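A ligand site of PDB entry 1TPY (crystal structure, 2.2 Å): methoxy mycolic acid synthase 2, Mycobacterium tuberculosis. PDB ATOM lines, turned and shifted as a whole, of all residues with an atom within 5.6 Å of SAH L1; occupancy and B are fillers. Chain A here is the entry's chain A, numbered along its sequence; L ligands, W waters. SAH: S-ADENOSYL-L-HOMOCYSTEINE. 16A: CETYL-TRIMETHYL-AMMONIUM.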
ATOM      1  N   PRO A   7      -5.176 -21.976  11.716  1.00  0.00           N
ATOM      2  CA  PRO A   7      -4.374 -21.600  10.543  1.00  0.00           C
ATOM      3  C   PRO A   7      -4.632 -20.212   9.967  1.00  0.00           C
ATOM      4  O   PRO A   7      -5.766 -19.712  10.002  1.00  0.00           O
ATOM      5  CB  PRO A   7      -4.695 -22.712   9.557  1.00  0.00           C
ATOM      6  CG  PRO A   7      -4.828 -23.907  10.441  1.00  0.00           C
ATOM      7  CD  PRO A   7      -5.669 -23.367  11.578  1.00  0.00           C
ATOM      8  N   HIS A   8      -3.586 -19.593   9.439  1.00  0.00           N
ATOM      9  CA  HIS A   8      -3.703 -18.277   8.823  1.00  0.00           C
ATOM     10  C   HIS A   8      -4.089 -18.470   7.362  1.00  0.00           C
ATOM     11  O   HIS A   8      -3.299 -18.185   6.453  1.00  0.00           O
ATOM     12  CB  HIS A   8      -2.372 -17.522   8.925  1.00  0.00           C
ATOM     13  CG  HIS A   8      -1.956 -17.203  10.322  1.00  0.00           C
ATOM     14  ND1 HIS A   8      -0.734 -17.561  10.850  1.00  0.00           N
ATOM     15  CD2 HIS A   8      -2.604 -16.531  11.312  1.00  0.00           C
ATOM     16  CE1 HIS A   8      -0.637 -17.128  12.090  1.00  0.00           C
ATOM     17  NE2 HIS A   8      -1.761 -16.499  12.396  1.00  0.00           N
ATOM     18  N   VAL A  12      -2.023 -16.837   3.673  1.00  0.00           N
ATOM     19  CA  VAL A  12      -1.416 -17.830   2.796  1.00  0.00           C
ATOM     20  C   VAL A  12      -2.183 -17.964   1.495  1.00  0.00           C
ATOM     21  O   VAL A  12      -1.576 -18.067   0.425  1.00  0.00           O
ATOM     22  CB  VAL A  12      -1.328 -19.213   3.496  1.00  0.00           C
ATOM     23  CG1 VAL A  12      -0.716 -20.254   2.562  1.00  0.00           C
ATOM     24  CG2 VAL A  12      -0.488 -19.093   4.766  1.00  0.00           C
ATOM     25  N   TYR A  16      -1.150 -18.165  -2.778  1.00  0.00           N
ATOM     26  CA  TYR A  16      -1.323 -19.412  -3.540  1.00  0.00           C
ATOM     27  C   TYR A  16      -2.649 -19.652  -4.235  1.00  0.00           C
ATOM     28  O   TYR A  16      -2.734 -20.540  -5.089  1.00  0.00           O
ATOM     29  CB  TYR A  16      -0.976 -20.616  -2.653  1.00  0.00           C
ATOM     30  CG  TYR A  16       0.368 -20.465  -2.000  1.00  0.00           C
ATOM     31  CD1 TYR A  16       0.495 -19.923  -0.725  1.00  0.00           C
ATOM     32  CD2 TYR A  16       1.535 -20.770  -2.707  1.00  0.00           C
ATOM     33  CE1 TYR A  16       1.733 -19.686  -0.161  1.00  0.00           C
ATOM     34  CE2 TYR A  16       2.784 -20.536  -2.145  1.00  0.00           C
ATOM     35  CZ  TYR A  16       2.876 -19.990  -0.881  1.00  0.00           C
ATOM     36  OH  TYR A  16       4.112 -19.729  -0.353  1.00  0.00           O
ATOM     37  N   GLN A  31       5.079 -27.739 -11.017  1.00  0.00           N
ATOM     38  CA  GLN A  31       4.532 -26.684 -10.180  1.00  0.00           C
ATOM     39  C   GLN A  31       5.173 -26.659  -8.789  1.00  0.00           C
ATOM     40  O   GLN A  31       4.530 -26.313  -7.794  1.00  0.00           O
ATOM     41  CB  GLN A  31       3.014 -26.834 -10.048  1.00  0.00           C
ATOM     42  CG  GLN A  31       2.271 -27.020 -11.368  1.00  0.00           C
ATOM     43  CD  GLN A  31       2.564 -25.911 -12.369  1.00  0.00           C
ATOM     44  OE1 GLN A  31       2.429 -24.723 -12.075  1.00  0.00           O
ATOM     45  NE2 GLN A  31       2.957 -26.307 -13.575  1.00  0.00           N
ATOM     46  N   THR A  32       6.442 -27.045  -8.716  1.00  0.00           N
ATOM     47  CA  THR A  32       7.160 -27.007  -7.457  1.00  0.00           C
ATOM     48  C   THR A  32       7.410 -25.515  -7.252  1.00  0.00           C
ATOM     49  O   THR A  32       7.739 -24.796  -8.183  1.00  0.00           O
ATOM     50  CB  THR A  32       8.499 -27.771  -7.528  1.00  0.00           C
ATOM     51  OG1 THR A  32       8.236 -29.156  -7.781  1.00  0.00           O
ATOM     52  CG2 THR A  32       9.259 -27.625  -6.227  1.00  0.00           C
ATOM     53  N   TYR A  33       7.236 -25.054  -6.018  1.00  0.00           N
ATOM     54  CA  TYR A  33       7.379 -23.643  -5.722  1.00  0.00           C
ATOM     55  C   TYR A  33       8.299 -23.475  -4.528  1.00  0.00           C
ATOM     56  O   TYR A  33       7.867 -23.110  -3.442  1.00  0.00           O
ATOM     57  CB  TYR A  33       5.986 -23.068  -5.441  1.00  0.00           C
ATOM     58  CG  TYR A  33       5.859 -21.570  -5.546  1.00  0.00           C
ATOM     59  CD1 TYR A  33       4.647 -20.944  -5.244  1.00  0.00           C
ATOM     60  CD2 TYR A  33       6.924 -20.767  -5.954  1.00  0.00           C
ATOM     61  CE1 TYR A  33       4.496 -19.576  -5.339  1.00  0.00           C
ATOM     62  CE2 TYR A  33       6.789 -19.380  -6.047  1.00  0.00           C
ATOM     63  CZ  TYR A  33       5.556 -18.792  -5.743  1.00  0.00           C
ATOM     64  OH  TYR A  33       5.383 -17.437  -5.828  1.00  0.00           O
ATOM     65  N   SER A  34       9.586 -23.751  -4.757  1.00  0.00           N
ATOM     66  CA  SER A  34      10.602 -23.665  -3.725  1.00  0.00           C
ATOM     67  C   SER A  34      11.969 -23.817  -4.404  1.00  0.00           C
ATOM     68  O   SER A  34      12.062 -24.237  -5.546  1.00  0.00           O
ATOM     69  CB  SER A  34      10.389 -24.784  -2.693  1.00  0.00           C
ATOM     70  OG  SER A  34      10.211 -26.042  -3.335  1.00  0.00           O
ATOM     71  N   LYS A  52      15.900 -31.563  -6.037  1.00  0.00           N
ATOM     72  CA  LYS A  52      15.679 -31.032  -4.685  1.00  0.00           C
ATOM     73  C   LYS A  52      14.708 -31.944  -3.914  1.00  0.00           C
ATOM     74  O   LYS A  52      14.898 -32.197  -2.727  1.00  0.00           O
ATOM     75  CB  LYS A  52      15.122 -29.601  -4.762  1.00  0.00           C
ATOM     76  CG  LYS A  52      14.642 -29.019  -3.435  1.00  0.00           C
ATOM     77  CD  LYS A  52      13.196 -29.407  -3.133  1.00  0.00           C
ATOM     78  CE  LYS A  52      12.239 -28.897  -4.216  1.00  0.00           C
ATOM     79  NZ  LYS A  52      12.303 -27.408  -4.399  1.00  0.00           N
ATOM     80  N   ASP A  70       3.391 -34.446   4.270  1.00  0.00           N
ATOM     81  CA  ASP A  70       4.007 -33.285   3.638  1.00  0.00           C
ATOM     82  C   ASP A  70       3.249 -32.067   4.139  1.00  0.00           C
ATOM     83  O   ASP A  70       2.139 -31.799   3.688  1.00  0.00           O
ATOM     84  CB  ASP A  70       3.910 -33.371   2.101  1.00  0.00           C
ATOM     85  CG  ASP A  70       4.552 -32.169   1.400  1.00  0.00           C
ATOM     86  OD1 ASP A  70       4.869 -31.182   2.090  1.00  0.00           O
ATOM     87  OD2 ASP A  70       4.752 -32.203   0.166  1.00  0.00           O
ATOM     88  N   ILE A  71       3.837 -31.339   5.089  1.00  0.00           N
ATOM     89  CA  ILE A  71       3.193 -30.144   5.644  1.00  0.00           C
ATOM     90  C   ILE A  71       3.464 -28.957   4.720  1.00  0.00           C
ATOM     91  O   ILE A  71       4.586 -28.451   4.656  1.00  0.00           O
ATOM     92  CB  ILE A  71       3.721 -29.857   7.055  1.00  0.00           C
ATOM     93  CG1 ILE A  71       3.485 -31.080   7.943  1.00  0.00           C
ATOM     94  CG2 ILE A  71       3.036 -28.612   7.645  1.00  0.00           C
ATOM     95  CD1 ILE A  71       4.008 -30.936   9.370  1.00  0.00           C
ATOM     96  N   GLY A  72       2.428 -28.528   4.005  1.00  0.00           N
ATOM     97  CA  GLY A  72       2.559 -27.434   3.056  1.00  0.00           C
ATOM     98  C   GLY A  72       2.967 -28.043   1.725  1.00  0.00           C
ATOM     99  O   GLY A  72       3.926 -27.599   1.095  1.00  0.00           O
ATOM    100  N   CYS A  73       2.211 -29.054   1.312  1.00  0.00           N
ATOM    101  CA  CYS A  73       2.462 -29.823   0.089  1.00  0.00           C
ATOM    102  C   CYS A  73       2.406 -29.087  -1.237  1.00  0.00           C
ATOM    103  O   CYS A  73       2.787 -29.638  -2.274  1.00  0.00           O
ATOM    104  CB  CYS A  73       1.491 -31.006   0.028  1.00  0.00           C
ATOM    105  SG  CYS A  73      -0.247 -30.504  -0.039  1.00  0.00           S
ATOM    106  N   GLY A  74       1.923 -27.851  -1.227  1.00  0.00           N
ATOM    107  CA  GLY A  74       1.841 -27.122  -2.480  1.00  0.00           C
ATOM    108  C   GLY A  74       0.970 -27.854  -3.482  1.00  0.00           C
ATOM    109  O   GLY A  74      -0.135 -28.277  -3.151  1.00  0.00           O
ATOM    110  N   TRP A  75       1.484 -28.004  -4.695  1.00  0.00           N
ATOM    111  CA  TRP A  75       0.742 -28.684  -5.757  1.00  0.00           C
ATOM    112  C   TRP A  75       0.990 -30.184  -5.848  1.00  0.00           C
ATOM    113  O   TRP A  75       0.722 -30.811  -6.873  1.00  0.00           O
ATOM    114  CB  TRP A  75       1.014 -27.990  -7.091  1.00  0.00           C
ATOM    115  CG  TRP A  75       0.233 -26.710  -7.252  1.00  0.00           C
ATOM    116  CD1 TRP A  75      -1.089 -26.594  -7.610  1.00  0.00           C
ATOM    117  CD2 TRP A  75       0.689 -25.375  -6.986  1.00  0.00           C
ATOM    118  NE1 TRP A  75      -1.468 -25.272  -7.584  1.00  0.00           N
ATOM    119  CE2 TRP A  75      -0.403 -24.504  -7.201  1.00  0.00           C
ATOM    120  CE3 TRP A  75       1.918 -24.831  -6.591  1.00  0.00           C
ATOM    121  CZ2 TRP A  75      -0.301 -23.116  -7.037  1.00  0.00           C
ATOM    122  CZ3 TRP A  75       2.019 -23.452  -6.425  1.00  0.00           C
ATOM    123  CH2 TRP A  75       0.905 -22.611  -6.650  1.00  0.00           C
ATOM    124  N   THR A  78       5.965 -33.267  -4.664  1.00  0.00           N
ATOM    125  CA  THR A  78       6.782 -33.984  -3.691  1.00  0.00           C
ATOM    126  C   THR A  78       6.125 -35.293  -3.263  1.00  0.00           C
ATOM    127  O   THR A  78       6.768 -36.342  -3.271  1.00  0.00           O
ATOM    128  CB  THR A  78       7.066 -33.110  -2.461  1.00  0.00           C
ATOM    129  OG1 THR A  78       7.804 -31.950  -2.865  1.00  0.00           O
ATOM    130  CG2 THR A  78       7.910 -33.893  -1.432  1.00  0.00           C
ATOM    131  N   LEU A  93      -0.841 -31.513   3.606  1.00  0.00           N
ATOM    132  CA  LEU A  93      -1.603 -30.438   4.208  1.00  0.00           C
ATOM    133  C   LEU A  93      -1.289 -29.135   3.494  1.00  0.00           C
ATOM    134  O   LEU A  93      -0.131 -28.870   3.165  1.00  0.00           O
ATOM    135  CB  LEU A  93      -1.234 -30.288   5.692  1.00  0.00           C
ATOM    136  CG  LEU A  93      -1.265 -31.536   6.575  1.00  0.00           C
ATOM    137  CD1 LEU A  93      -0.797 -31.162   7.988  1.00  0.00           C
ATOM    138  CD2 LEU A  93      -2.673 -32.124   6.615  1.00  0.00           C
ATOM    139  N   THR A  94      -2.319 -28.342   3.232  1.00  0.00           N
ATOM    140  CA  THR A  94      -2.143 -27.056   2.584  1.00  0.00           C
ATOM    141  C   THR A  94      -3.296 -26.133   2.952  1.00  0.00           C
ATOM    142  O   THR A  94      -4.415 -26.580   3.217  1.00  0.00           O
ATOM    143  CB  THR A  94      -2.061 -27.193   1.045  1.00  0.00           C
ATOM    144  OG1 THR A  94      -1.916 -25.893   0.468  1.00  0.00           O
ATOM    145  CG2 THR A  94      -3.321 -27.862   0.502  1.00  0.00           C
ATOM    146  N   LEU A  95      -3.016 -24.836   2.993  1.00  0.00           N
ATOM    147  CA  LEU A  95      -4.033 -23.855   3.329  1.00  0.00           C
ATOM    148  C   LEU A  95      -4.619 -23.263   2.054  1.00  0.00           C
ATOM    149  O   LEU A  95      -5.531 -22.441   2.100  1.00  0.00           O
ATOM    150  CB  LEU A  95      -3.406 -22.749   4.179  1.00  0.00           C
ATOM    151  CG  LEU A  95      -2.689 -23.214   5.444  1.00  0.00           C
ATOM    152  CD1 LEU A  95      -2.199 -21.992   6.219  1.00  0.00           C
ATOM    153  CD2 LEU A  95      -3.634 -24.046   6.309  1.00  0.00           C
ATOM    154  N   SER A  96      -4.078 -23.694   0.925  1.00  0.00           N
ATOM    155  CA  SER A  96      -4.516 -23.227  -0.383  1.00  0.00           C
ATOM    156  C   SER A  96      -5.644 -24.065  -0.979  1.00  0.00           C
ATOM    157  O   SER A  96      -5.499 -25.263  -1.179  1.00  0.00           O
ATOM    158  CB  SER A  96      -3.336 -23.210  -1.354  1.00  0.00           C
ATOM    159  OG  SER A  96      -3.800 -23.187  -2.691  1.00  0.00           O
ATOM    160  N   GLN A  99      -4.609 -25.446  -4.401  1.00  0.00           N
ATOM    161  CA  GLN A  99      -3.656 -26.533  -4.285  1.00  0.00           C
ATOM    162  C   GLN A  99      -4.336 -27.822  -3.844  1.00  0.00           C
ATOM    163  O   GLN A  99      -4.016 -28.898  -4.331  1.00  0.00           O
ATOM    164  CB  GLN A  99      -2.521 -26.153  -3.323  1.00  0.00           C
ATOM    165  CG  GLN A  99      -1.517 -25.172  -3.957  1.00  0.00           C
ATOM    166  CD  GLN A  99      -0.454 -24.678  -2.982  1.00  0.00           C
ATOM    167  OE1 GLN A  99       0.538 -24.059  -3.387  1.00  0.00           O
ATOM    168  NE2 GLN A  99      -0.661 -24.938  -1.704  1.00  0.00           N
ATOM    169  N   ALA A 121      -6.016 -27.899   5.402  1.00  0.00           N
ATOM    170  CA  ALA A 121      -5.836 -27.647   6.830  1.00  0.00           C
ATOM    171  C   ALA A 121      -4.381 -27.371   7.150  1.00  0.00           C
ATOM    172  O   ALA A 121      -3.487 -27.641   6.341  1.00  0.00           O
ATOM    173  CB  ALA A 121      -6.322 -28.871   7.624  1.00  0.00           C
ATOM    174  N   GLY A 122      -4.126 -26.818   8.331  1.00  0.00           N
ATOM    175  CA  GLY A 122      -2.759 -26.537   8.720  1.00  0.00           C
ATOM    176  C   GLY A 122      -2.247 -27.667   9.585  1.00  0.00           C
ATOM    177  O   GLY A 122      -3.006 -28.559   9.947  1.00  0.00           O
ATOM    178  N   TRP A 123      -0.955 -27.644   9.884  1.00  0.00           N
ATOM    179  CA  TRP A 123      -0.407 -28.679  10.742  1.00  0.00           C
ATOM    180  C   TRP A 123      -1.076 -28.522  12.097  1.00  0.00           C
ATOM    181  O   TRP A 123      -1.312 -29.506  12.804  1.00  0.00           O
ATOM    182  CB  TRP A 123       1.117 -28.517  10.914  1.00  0.00           C
ATOM    183  CG  TRP A 123       1.523 -27.130  11.345  1.00  0.00           C
ATOM    184  CD1 TRP A 123       1.838 -26.083  10.539  1.00  0.00           C
ATOM    185  CD2 TRP A 123       1.598 -26.645  12.689  1.00  0.00           C
ATOM    186  NE1 TRP A 123       2.112 -24.965  11.293  1.00  0.00           N
ATOM    187  CE2 TRP A 123       1.965 -25.279  12.616  1.00  0.00           C
ATOM    188  CE3 TRP A 123       1.385 -27.212  13.950  1.00  0.00           C
ATOM    189  CZ2 TRP A 123       2.127 -24.485  13.749  1.00  0.00           C
ATOM    190  CZ3 TRP A 123       1.547 -26.418  15.084  1.00  0.00           C
ATOM    191  CH2 TRP A 123       1.910 -25.072  14.973  1.00  0.00           C
ATOM    192  N   GLU A 124      -1.391 -27.286  12.469  1.00  0.00           N
ATOM    193  CA  GLU A 124      -2.012 -27.060  13.766  1.00  0.00           C
ATOM    194  C   GLU A 124      -3.336 -27.812  13.937  1.00  0.00           C
ATOM    195  O   GLU A 124      -3.801 -28.011  15.060  1.00  0.00           O
ATOM    196  CB  GLU A 124      -2.188 -25.543  14.034  1.00  0.00           C
ATOM    197  CG  GLU A 124      -2.574 -24.650  12.877  1.00  0.00           C
ATOM    198  CD  GLU A 124      -1.385 -24.175  12.022  1.00  0.00           C
ATOM    199  OE1 GLU A 124      -0.903 -24.972  11.190  1.00  0.00           O
ATOM    200  OE2 GLU A 124      -0.941 -23.020  12.187  1.00  0.00           O
ATOM    201  N   SER A 135       8.709 -30.945   4.828  1.00  0.00           N
ATOM    202  CA  SER A 135       8.089 -29.643   4.730  1.00  0.00           C
ATOM    203  C   SER A 135       9.080 -28.751   4.021  1.00  0.00           C
ATOM    204  O   SER A 135      10.159 -28.462   4.529  1.00  0.00           O
ATOM    205  CB  SER A 135       7.770 -29.071   6.115  1.00  0.00           C
ATOM    206  OG  SER A 135       7.050 -27.862   5.980  1.00  0.00           O
ATOM    207  N   ILE A 136       8.705 -28.313   2.825  1.00  0.00           N
ATOM    208  CA  ILE A 136       9.551 -27.491   2.002  1.00  0.00           C
ATOM    209  C   ILE A 136       8.906 -26.154   1.683  1.00  0.00           C
ATOM    210  O   ILE A 136       7.863 -26.109   1.029  1.00  0.00           O
ATOM    211  CB  ILE A 136       9.872 -28.235   0.690  1.00  0.00           C
ATOM    212  CG1 ILE A 136      10.525 -29.584   1.010  1.00  0.00           C
ATOM    213  CG2 ILE A 136      10.775 -27.378  -0.198  1.00  0.00           C
ATOM    214  CD1 ILE A 136      10.578 -30.529  -0.163  1.00  0.00           C
ATOM    215  N   GLY A 137       9.528 -25.082   2.137  1.00  0.00           N
ATOM    216  CA  GLY A 137       9.011 -23.751   1.864  1.00  0.00           C
ATOM    217  C   GLY A 137       7.699 -23.393   2.531  1.00  0.00           C
ATOM    218  O   GLY A 137       7.017 -22.456   2.093  1.00  0.00           O
ATOM    219  N   ALA A 138       7.328 -24.104   3.580  1.00  0.00           N
ATOM    220  CA  ALA A 138       6.078 -23.824   4.285  1.00  0.00           C
ATOM    221  C   ALA A 138       6.341 -23.102   5.602  1.00  0.00           C
ATOM    222  O   ALA A 138       5.601 -22.194   5.973  1.00  0.00           O
ATOM    223  CB  ALA A 138       5.317 -25.121   4.541  1.00  0.00           C
ATOM    224  N   HIS A 141       5.923 -19.392   6.557  1.00  0.00           N
ATOM    225  CA  HIS A 141       4.560 -18.906   6.760  1.00  0.00           C
ATOM    226  C   HIS A 141       4.029 -19.153   8.178  1.00  0.00           C
ATOM    227  O   HIS A 141       3.101 -18.482   8.618  1.00  0.00           O
ATOM    228  CB  HIS A 141       3.594 -19.588   5.789  1.00  0.00           C
ATOM    229  CG  HIS A 141       3.735 -19.128   4.368  1.00  0.00           C
ATOM    230  ND1 HIS A 141       3.338 -17.882   3.946  1.00  0.00           N
ATOM    231  CD2 HIS A 141       4.207 -19.766   3.277  1.00  0.00           C
ATOM    232  CE1 HIS A 141       3.562 -17.769   2.647  1.00  0.00           C
ATOM    233  NE2 HIS A 141       4.087 -18.895   2.222  1.00  0.00           N
ATOM    234  N   PHE A 142       4.609 -20.119   8.875  1.00  0.00           N
ATOM    235  CA  PHE A 142       4.152 -20.479  10.206  1.00  0.00           C
ATOM    236  C   PHE A 142       4.069 -19.336  11.214  1.00  0.00           C
ATOM    237  O   PHE A 142       3.133 -19.280  12.011  1.00  0.00           O
ATOM    238  CB  PHE A 142       5.033 -21.592  10.784  1.00  0.00           C
ATOM    239  CG  PHE A 142       4.927 -22.898  10.055  1.00  0.00           C
ATOM    240  CD1 PHE A 142       5.734 -23.966  10.414  1.00  0.00           C
ATOM    241  CD2 PHE A 142       4.060 -23.051   8.969  1.00  0.00           C
ATOM    242  CE1 PHE A 142       5.684 -25.172   9.713  1.00  0.00           C
ATOM    243  CE2 PHE A 142       4.003 -24.245   8.268  1.00  0.00           C
ATOM    244  CZ  PHE A 142       4.820 -25.323   8.637  1.00  0.00           C
HETATM  245  N   SAH L   1       6.045 -27.628  -0.421  1.00  0.00           N
HETATM  246  CA  SAH L   1       5.625 -27.159  -1.746  1.00  0.00           C
HETATM  247  CB  SAH L   1       4.848 -25.828  -1.652  1.00  0.00           C
HETATM  248  CG  SAH L   1       5.529 -24.632  -0.984  1.00  0.00           C
HETATM  249  SD  SAH L   1       4.502 -23.136  -0.961  1.00  0.00           S
HETATM  250  C   SAH L   1       6.829 -26.988  -2.667  1.00  0.00           C
HETATM  251  O   SAH L   1       7.972 -27.097  -2.180  1.00  0.00           O
HETATM  252  OXT SAH L   1       6.619 -26.748  -3.877  1.00  0.00           O
HETATM  253  C5' SAH L   1       4.072 -22.987   0.790  1.00  0.00           C
HETATM  254  C4' SAH L   1       3.090 -24.103   1.198  1.00  0.00           C
HETATM  255  O4' SAH L   1       2.976 -24.250   2.629  1.00  0.00           O
HETATM  256  C3' SAH L   1       1.672 -23.878   0.679  1.00  0.00           C
HETATM  257  O3' SAH L   1       1.143 -25.125   0.197  1.00  0.00           O
HETATM  258  C2' SAH L   1       0.932 -23.394   1.892  1.00  0.00           C
HETATM  259  O2' SAH L   1      -0.489 -23.617   1.774  1.00  0.00           O
HETATM  260  C1' SAH L   1       1.590 -24.198   2.970  1.00  0.00           C
HETATM  261  N9  SAH L   1       1.385 -23.666   4.381  1.00  0.00           N
HETATM  262  C8  SAH L   1       1.623 -22.445   4.926  1.00  0.00           C
HETATM  263  N7  SAH L   1       1.353 -22.306   6.183  1.00  0.00           N
HETATM  264  C5  SAH L   1       0.879 -23.571   6.526  1.00  0.00           C
HETATM  265  C6  SAH L   1       0.404 -24.147   7.731  1.00  0.00           C
HETATM  266  N6  SAH L   1       0.322 -23.466   8.875  1.00  0.00           N
HETATM  267  N1  SAH L   1       0.001 -25.467   7.701  1.00  0.00           N
HETATM  268  C2  SAH L   1       0.076 -26.169   6.552  1.00  0.00           C
HETATM  269  N3  SAH L   1       0.504 -25.728   5.353  1.00  0.00           N
HETATM  270  C4  SAH L   1       0.895 -24.407   5.419  1.00  0.00           C
HETATM  271  C1  16A L   2      11.018 -17.269  -3.608  1.00  0.00           C
HETATM  272  C2  16A L   2      10.608 -16.546  -2.328  1.00  0.00           C
HETATM  273  C3  16A L   2      11.825 -15.837  -1.705  1.00  0.00           C
HETATM  274  C4  16A L   2      11.539 -15.055  -0.421  1.00  0.00           C
HETATM  275  C5  16A L   2      12.843 -14.408   0.071  1.00  0.00           C
HETATM  276  C6  16A L   2      12.723 -13.578   1.359  1.00  0.00           C
HETATM  277  C7  16A L   2      11.849 -12.304   1.344  1.00  0.00           C
HETATM  278  C8  16A L   2      11.358 -11.745   2.699  1.00  0.00           C
HETATM  279  C9  16A L   2      10.660 -12.742   3.667  1.00  0.00           C
HETATM  280  C10 16A L   2       9.332 -13.362   3.178  1.00  0.00           C
HETATM  281  C11 16A L   2       8.888 -14.668   3.890  1.00  0.00           C
HETATM  282  C12 16A L   2       7.838 -15.500   3.132  1.00  0.00           C
HETATM  283  C13 16A L   2       8.463 -16.690   2.412  1.00  0.00           C
HETATM  284  C14 16A L   2       7.427 -17.456   1.595  1.00  0.00           C
HETATM  285  C15 16A L   2       8.189 -18.455   0.702  1.00  0.00           C
HETATM  286  C16 16A L   2       7.180 -19.122  -0.247  1.00  0.00           C
HETATM  287  N1  16A L   2       7.478 -20.152  -1.331  1.00  0.00           N
HETATM  288  C17 16A L   2       6.603 -20.681  -2.198  1.00  0.00           C
HETATM  289  C18 16A L   2       8.603 -19.674  -2.230  1.00  0.00           C
HETATM  290  C19 16A L   2       8.019 -21.404  -0.676  1.00  0.00           C
HETATM  291  O   HOH W   1       9.033 -29.260  -3.251  1.00  0.00           O
HETATM  292  O   HOH W   2      -1.048 -20.936  10.134  1.00  0.00           O
HETATM  293  O   HOH W   3       6.129 -28.879   1.999  1.00  0.00           O
HETATM  294  O   HOH W   4       4.436 -27.415  -5.315  1.00  0.00           O
HETATM  295  O   HOH W   5       6.307 -30.329  -1.181  1.00  0.00           O
HETATM  296  O   HOH W   6       0.891 -20.726   8.194  1.00  0.00           O
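A nitrogen (N) of SAH L1 lies within hydrogen-bond range of the backbone carbonyl oxygen of Gly 72 (2.6 Å). The side-chain amide nitrogen (NE2) of Gln 99 is in hydrogen-bond range of an oxygen (O3') of SAH L1. O of SAH L1 lies within hydrogen-bond range of OG of Ser 34, 2.7 Å away. A nitrogen (N) of SAH L1 lies within hydrogen-bond range of the backbone carbonyl oxygen (O) of Ile 136 (2.8 Å). An oxygen (OXT) of SAH L1 is in hydrogen-bond range of the backbone NH of Tyr 33, 2.8 Å away. O2' of SAH L1 lies within hydrogen-bond range of OG1 of Thr 94 (3.0 Å). OE1 of Glu 124 lies within hydrogen-bond range of N6 of SAH L1 (3.0 Å). The backbone NH of Leu 95 sits at hydrogen-bond distance from an oxygen (O2') of SAH L1, at 3.1 Å. N of Gly 74 sits at hydrogen-bond distance from O3' of SAH L1 (3.2 Å). The backbone NH (N) of Trp 123 lies within hydrogen-bond range of a nitrogen (N1) of SAH L1, at 3.2 Å. The side-chain hydroxyl of Tyr 16 lies close to a sulfur (SD) of SAH L1 (3.5 Å).
NE2 of Gln 99 lies within hydrogen-bond range of OG1 of Thr 94, 2.7 Å away. The side-chain hydroxyl of Ser 34 sits at hydrogen-bond distance from the side-chain amino group of Lys 52, 2.7 Å away. OG1 of Thr 94 is in hydrogen-bond range of N of Ser 96, at 3.1 Å. N of Ala 121 is in hydrogen-bond range of O of Thr 94 (3.0 Å). NE1 of Trp 123 is in hydrogen-bond range of OE1 of Glu 124 (3.0 Å). A ring nitrogen (NE2) of His 141 is in hydrogen-bond range of the side-chain hydroxyl of Tyr 16 (2.7 Å). The side-chain carboxylate (OD1) of Asp 70 lies close to the backbone NH (N) of Cys 73 (3.5 Å). The backbone NH (N) of Leu 93 lies within hydrogen-bond range of the backbone carbonyl oxygen (O) of Asp 70 (3.0 Å).
CG1 of Val 12 touches O2' of SAH L1, 3.5 Å away. Thr 32 touches SAH L1 (CA to OXT, 3.6 Å). CG2 of Ile 71 touches C2 of SAH L1 (3.99 Å). Cys 73 touches SAH L1 (C to CA, 3.8 Å). Leu 93 touches SAH L1. Ser 96 touches SAH L1. O of Ala 121 touches C2 of SAH L1, at 3.9 Å. Gly 122 touches SAH L1. Gly 137 touches SAH L1 (O to C5', 3.3 Å). Ala 138 touches SAH L1 (CB to O4', 3.1 Å). CB of His 141 touches N7 of SAH L1, at 3.5 Å. Phe 142 touches SAH L1. Hydrophobic or aromatic side chains within 4 Å of SAH L1: Val 12, Tyr 16, Ile 71, Leu 95, Trp 123, Ile 136, Ala 138, His 141 and Phe 142. Within 4 Å of SAH L1: Val 12, Tyr 16, Thr 32, Tyr 33, Ser 34, Ile 71, Gly 72, Cys 73, Gly 74, Leu 93, Thr 94, Leu 95, Ser 96, Gln 99, Ala 121, Gly 122, Trp 123, Glu 124, Ile 136, Gly 137, Ala 138, His 141 and Phe 142. The nearest printed residue that does not touch SAH L1 is Gln 31 (4.5 Å).
Water W6 bridges a nitrogen (N7) of SAH L1 (2.6 Å) and the backbone carbonyl oxygen (O) of His 141 (3.2 Å). Water W1 lies within hydrogen-bond range of an oxygen (O) of SAH L1 (2.6 Å), the side-chain hydroxyl (OG1) of Thr 78 (3.0 Å) and the side-chain hydroxyl (OG) of Ser 34 (3.4 Å). Water W4 lies within hydrogen-bond range of OXT of SAH L1 (2.7 Å), O of Gln 31 (2.7 Å) and N of Trp 75 (3.1 Å). Water W5 lies within hydrogen-bond range of OG1 of Thr 78 (2.8 Å), OD2 of Asp 70 (2.8 Å) and N of SAH L1 (2.8 Å). Water W2 lies within hydrogen-bond range of OE2 of Glu 124, N of His 8 and N6 of SAH L1.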
